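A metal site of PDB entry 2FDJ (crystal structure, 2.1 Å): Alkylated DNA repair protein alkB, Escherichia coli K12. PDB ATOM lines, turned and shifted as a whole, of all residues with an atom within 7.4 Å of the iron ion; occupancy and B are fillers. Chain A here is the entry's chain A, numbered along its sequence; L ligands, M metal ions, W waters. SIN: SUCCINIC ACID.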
ATOM      1  N   LEU A 108     -33.809 -19.414 -32.780  1.00  0.00           N
ATOM      2  CA  LEU A 108     -34.642 -18.643 -31.864  1.00  0.00           C
ATOM      3  C   LEU A 108     -34.848 -17.291 -32.524  1.00  0.00           C
ATOM      4  O   LEU A 108     -33.873 -16.630 -32.902  1.00  0.00           O
ATOM      5  CB  LEU A 108     -33.943 -18.483 -30.508  1.00  0.00           C
ATOM      6  CG  LEU A 108     -34.629 -17.646 -29.423  1.00  0.00           C
ATOM      7  CD1 LEU A 108     -36.009 -18.207 -29.078  1.00  0.00           C
ATOM      8  CD2 LEU A 108     -33.748 -17.619 -28.203  1.00  0.00           C
ATOM      9  N   ASN A 110     -36.154 -13.571 -32.059  1.00  0.00           N
ATOM     10  CA  ASN A 110     -36.498 -12.541 -31.074  1.00  0.00           C
ATOM     11  C   ASN A 110     -37.035 -11.274 -31.728  1.00  0.00           C
ATOM     12  O   ASN A 110     -36.486 -10.806 -32.728  1.00  0.00           O
ATOM     13  CB  ASN A 110     -35.271 -12.181 -30.233  1.00  0.00           C
ATOM     14  CG  ASN A 110     -34.842 -13.278 -29.278  1.00  0.00           C
ATOM     15  OD1 ASN A 110     -33.893 -13.111 -28.529  1.00  0.00           O
ATOM     16  ND2 ASN A 110     -35.540 -14.396 -29.294  1.00  0.00           N
ATOM     17  N   LEU A 118     -33.067  -7.586 -23.110  1.00  0.00           N
ATOM     18  CA  LEU A 118     -32.800  -8.974 -22.759  1.00  0.00           C
ATOM     19  C   LEU A 118     -31.758  -8.923 -21.660  1.00  0.00           C
ATOM     20  O   LEU A 118     -30.667  -8.401 -21.862  1.00  0.00           O
ATOM     21  CB  LEU A 118     -32.215  -9.720 -23.962  1.00  0.00           C
ATOM     22  CG  LEU A 118     -32.850 -11.023 -24.436  1.00  0.00           C
ATOM     23  CD1 LEU A 118     -31.879 -11.695 -25.395  1.00  0.00           C
ATOM     24  CD2 LEU A 118     -33.164 -11.950 -23.290  1.00  0.00           C
ATOM     25  N   SER A 119     -32.078  -9.466 -20.488  1.00  0.00           N
ATOM     26  CA  SER A 119     -31.134  -9.456 -19.382  1.00  0.00           C
ATOM     27  C   SER A 119     -29.950 -10.371 -19.642  1.00  0.00           C
ATOM     28  O   SER A 119     -30.012 -11.269 -20.480  1.00  0.00           O
ATOM     29  CB  SER A 119     -31.830  -9.828 -18.060  1.00  0.00           C
ATOM     30  OG  SER A 119     -32.342 -11.146 -18.069  1.00  0.00           O
ATOM     31  N   HIS A 121     -27.235 -13.133 -19.817  1.00  0.00           N
ATOM     32  CA  HIS A 121     -27.355 -14.588 -19.782  1.00  0.00           C
ATOM     33  C   HIS A 121     -26.292 -15.213 -20.677  1.00  0.00           C
ATOM     34  O   HIS A 121     -25.658 -14.552 -21.509  1.00  0.00           O
ATOM     35  CB  HIS A 121     -28.735 -15.006 -20.322  1.00  0.00           C
ATOM     36  CG  HIS A 121     -28.888 -14.786 -21.795  1.00  0.00           C
ATOM     37  ND1 HIS A 121     -29.131 -13.530 -22.329  1.00  0.00           N
ATOM     38  CD2 HIS A 121     -28.800 -15.627 -22.841  1.00  0.00           C
ATOM     39  CE1 HIS A 121     -29.177 -13.627 -23.649  1.00  0.00           C
ATOM     40  NE2 HIS A 121     -28.971 -14.892 -23.978  1.00  0.00           N
ATOM     41  N   GLN A 122     -26.129 -16.528 -20.517  1.00  0.00           N
ATOM     42  CA  GLN A 122     -25.186 -17.291 -21.323  1.00  0.00           C
ATOM     43  C   GLN A 122     -25.999 -18.345 -22.064  1.00  0.00           C
ATOM     44  O   GLN A 122     -27.031 -18.796 -21.567  1.00  0.00           O
ATOM     45  CB  GLN A 122     -24.185 -18.035 -20.436  1.00  0.00           C
ATOM     46  CG  GLN A 122     -23.119 -17.187 -19.784  1.00  0.00           C
ATOM     47  CD  GLN A 122     -22.265 -18.012 -18.831  1.00  0.00           C
ATOM     48  OE1 GLN A 122     -22.783 -18.655 -17.917  1.00  0.00           O
ATOM     49  NE2 GLN A 122     -20.958 -18.014 -19.043  1.00  0.00           N
ATOM     50  N   ASP A 123     -25.532 -18.716 -23.257  1.00  0.00           N
ATOM     51  CA  ASP A 123     -26.184 -19.754 -24.048  1.00  0.00           C
ATOM     52  C   ASP A 123     -25.440 -21.033 -23.656  1.00  0.00           C
ATOM     53  O   ASP A 123     -24.391 -21.339 -24.232  1.00  0.00           O
ATOM     54  CB  ASP A 123     -25.985 -19.503 -25.539  1.00  0.00           C
ATOM     55  CG  ASP A 123     -26.372 -18.105 -25.977  1.00  0.00           C
ATOM     56  OD1 ASP A 123     -27.320 -17.519 -25.411  1.00  0.00           O
ATOM     57  OD2 ASP A 123     -25.716 -17.591 -26.911  1.00  0.00           O
ATOM     58  N   ILE A 133     -22.725 -19.944 -32.395  1.00  0.00           N
ATOM     59  CA  ILE A 133     -24.091 -19.460 -32.495  1.00  0.00           C
ATOM     60  C   ILE A 133     -24.006 -18.298 -33.476  1.00  0.00           C
ATOM     61  O   ILE A 133     -23.188 -17.387 -33.296  1.00  0.00           O
ATOM     62  CB  ILE A 133     -24.667 -19.000 -31.138  1.00  0.00           C
ATOM     63  CG1 ILE A 133     -25.027 -20.236 -30.298  1.00  0.00           C
ATOM     64  CG2 ILE A 133     -25.885 -18.097 -31.333  1.00  0.00           C
ATOM     65  CD1 ILE A 133     -25.652 -19.927 -28.969  1.00  0.00           C
ATOM     66  N   PHE A 144     -25.785  -4.203 -28.171  1.00  0.00           N
ATOM     67  CA  PHE A 144     -25.496  -5.531 -27.641  1.00  0.00           C
ATOM     68  C   PHE A 144     -24.372  -5.424 -26.616  1.00  0.00           C
ATOM     69  O   PHE A 144     -23.336  -4.828 -26.881  1.00  0.00           O
ATOM     70  CB  PHE A 144     -25.060  -6.452 -28.775  1.00  0.00           C
ATOM     71  CG  PHE A 144     -24.684  -7.840 -28.351  1.00  0.00           C
ATOM     72  CD1 PHE A 144     -25.649  -8.853 -28.285  1.00  0.00           C
ATOM     73  CD2 PHE A 144     -23.362  -8.155 -28.020  1.00  0.00           C
ATOM     74  CE1 PHE A 144     -25.307 -10.148 -27.912  1.00  0.00           C
ATOM     75  CE2 PHE A 144     -23.006  -9.451 -27.645  1.00  0.00           C
ATOM     76  CZ  PHE A 144     -23.975 -10.449 -27.596  1.00  0.00           C
ATOM     77  N   PHE A 175     -19.611 -16.210 -23.463  1.00  0.00           N
ATOM     78  CA  PHE A 175     -19.784 -14.925 -22.796  1.00  0.00           C
ATOM     79  C   PHE A 175     -21.205 -14.606 -22.348  1.00  0.00           C
ATOM     80  O   PHE A 175     -22.188 -15.003 -23.000  1.00  0.00           O
ATOM     81  CB  PHE A 175     -19.298 -13.778 -23.690  1.00  0.00           C
ATOM     82  CG  PHE A 175     -17.801 -13.686 -23.840  1.00  0.00           C
ATOM     83  CD1 PHE A 175     -17.235 -12.806 -24.766  1.00  0.00           C
ATOM     84  CD2 PHE A 175     -16.951 -14.458 -23.043  1.00  0.00           C
ATOM     85  CE1 PHE A 175     -15.847 -12.697 -24.900  1.00  0.00           C
ATOM     86  CE2 PHE A 175     -15.572 -14.353 -23.173  1.00  0.00           C
ATOM     87  CZ  PHE A 175     -15.020 -13.473 -24.102  1.00  0.00           C
ATOM     88  N   HIS A 177     -24.224 -12.191 -22.025  1.00  0.00           N
ATOM     89  CA  HIS A 177     -24.620 -11.124 -22.940  1.00  0.00           C
ATOM     90  C   HIS A 177     -26.085 -10.735 -22.814  1.00  0.00           C
ATOM     91  O   HIS A 177     -26.869 -11.433 -22.156  1.00  0.00           O
ATOM     92  CB  HIS A 177     -24.327 -11.536 -24.383  1.00  0.00           C
ATOM     93  CG  HIS A 177     -24.996 -12.801 -24.813  1.00  0.00           C
ATOM     94  ND1 HIS A 177     -24.445 -14.041 -24.578  1.00  0.00           N
ATOM     95  CD2 HIS A 177     -26.176 -13.026 -25.422  1.00  0.00           C
ATOM     96  CE1 HIS A 177     -25.259 -14.983 -25.032  1.00  0.00           C
ATOM     97  NE2 HIS A 177     -26.324 -14.386 -25.549  1.00  0.00           N
ATOM     98  N   GLY A 178     -26.441  -9.623 -23.453  1.00  0.00           N
ATOM     99  CA  GLY A 178     -27.812  -9.141 -23.412  1.00  0.00           C
ATOM    100  C   GLY A 178     -28.032  -7.996 -24.388  1.00  0.00           C
ATOM    101  O   GLY A 178     -27.147  -7.659 -25.152  1.00  0.00           O
ATOM    102  N   ASN A 196     -34.105 -10.557 -34.330  1.00  0.00           N
ATOM    103  CA  ASN A 196     -32.807 -11.185 -34.191  1.00  0.00           C
ATOM    104  C   ASN A 196     -32.984 -12.677 -34.287  1.00  0.00           C
ATOM    105  O   ASN A 196     -33.862 -13.247 -33.618  1.00  0.00           O
ATOM    106  CB  ASN A 196     -32.097 -10.823 -32.887  1.00  0.00           C
ATOM    107  CG  ASN A 196     -30.713 -11.479 -32.798  1.00  0.00           C
ATOM    108  OD1 ASN A 196     -30.573 -12.573 -32.263  1.00  0.00           O
ATOM    109  ND2 ASN A 196     -29.710 -10.815 -33.364  1.00  0.00           N
ATOM    110  N   THR A 198     -31.009 -16.344 -33.896  1.00  0.00           N
ATOM    111  CA  THR A 198     -29.825 -17.000 -33.344  1.00  0.00           C
ATOM    112  C   THR A 198     -29.877 -18.487 -33.652  1.00  0.00           C
ATOM    113  O   THR A 198     -30.714 -19.213 -33.107  1.00  0.00           O
ATOM    114  CB  THR A 198     -29.624 -16.754 -31.828  1.00  0.00           C
ATOM    115  OG1 THR A 198     -30.869 -16.788 -31.147  1.00  0.00           O
ATOM    116  CG2 THR A 198     -28.932 -15.416 -31.576  1.00  0.00           C
ATOM    117  N   ARG A 200     -28.670 -22.261 -33.675  1.00  0.00           N
ATOM    118  CA  ARG A 200     -27.990 -23.148 -32.744  1.00  0.00           C
ATOM    119  C   ARG A 200     -28.074 -24.605 -33.138  1.00  0.00           C
ATOM    120  O   ARG A 200     -29.057 -25.048 -33.734  1.00  0.00           O
ATOM    121  CB  ARG A 200     -28.615 -23.035 -31.337  1.00  0.00           C
ATOM    122  CG  ARG A 200     -28.707 -21.656 -30.759  1.00  0.00           C
ATOM    123  CD  ARG A 200     -30.156 -21.188 -30.693  1.00  0.00           C
ATOM    124  NE  ARG A 200     -30.267 -19.804 -30.247  1.00  0.00           N
ATOM    125  CZ  ARG A 200     -30.219 -19.415 -28.978  1.00  0.00           C
ATOM    126  NH1 ARG A 200     -30.072 -20.297 -28.012  1.00  0.00           N
ATOM    127  NH2 ARG A 200     -30.279 -18.117 -28.690  1.00  0.00           N
HETATM  128  C1  SIN L   1     -30.145 -13.571 -27.774  1.00  0.00           C
HETATM  129  O1  SIN L   1     -29.126 -13.559 -27.113  1.00  0.00           O
HETATM  130  O2  SIN L   1     -31.110 -14.488 -27.511  1.00  0.00           O
HETATM  131  C2  SIN L   1     -30.417 -12.499 -28.807  1.00  0.00           C
HETATM  132  C3  SIN L   1     -29.330 -11.418 -28.803  1.00  0.00           C
HETATM  133  C4  SIN L   1     -29.696 -10.337 -29.794  1.00  0.00           C
HETATM  134  O3  SIN L   1     -30.848 -10.032 -29.957  1.00  0.00           O
HETATM  135  O4  SIN L   1     -28.768  -9.806 -30.598  1.00  0.00           O
HETATM  136 FE    FE M   1     -28.287 -15.501 -25.941  1.00  0.00          FE
HETATM  137  O   HOH W   1     -27.858 -16.277 -28.072  1.00  0.00           O
HETATM  138  O   HOH W   2     -30.134 -16.542 -26.145  1.00  0.00           O
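ND1 of His 121 sits at hydrogen-bond distance from O of Ser 119 (3.1 Å). The backbone carbonyl oxygen (O) of Phe 175 sits at hydrogen-bond distance from a ring nitrogen (ND1) of His 177, 2.9 Å away.
Water W2 is bound to the iron ion (2.1 Å). NE2 of His 121 is bound to the iron ion (2.2 Å). A ring nitrogen (NE2) of His 177 is bound to the iron ion, at 2.3 Å. OD1 of Asp 123 binds the iron ion, at 2.3 Å. The iron ion is bound by water W1, at 2.3 Å. O1 of the ligand is bound to the iron ion.
Water W1 lies within hydrogen-bond range of the side-chain carboxylate of Asp 123 and the guanidinium group of Arg 200.
Of the 15 residues printed, 3 come within 4 Å of the iron ion.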
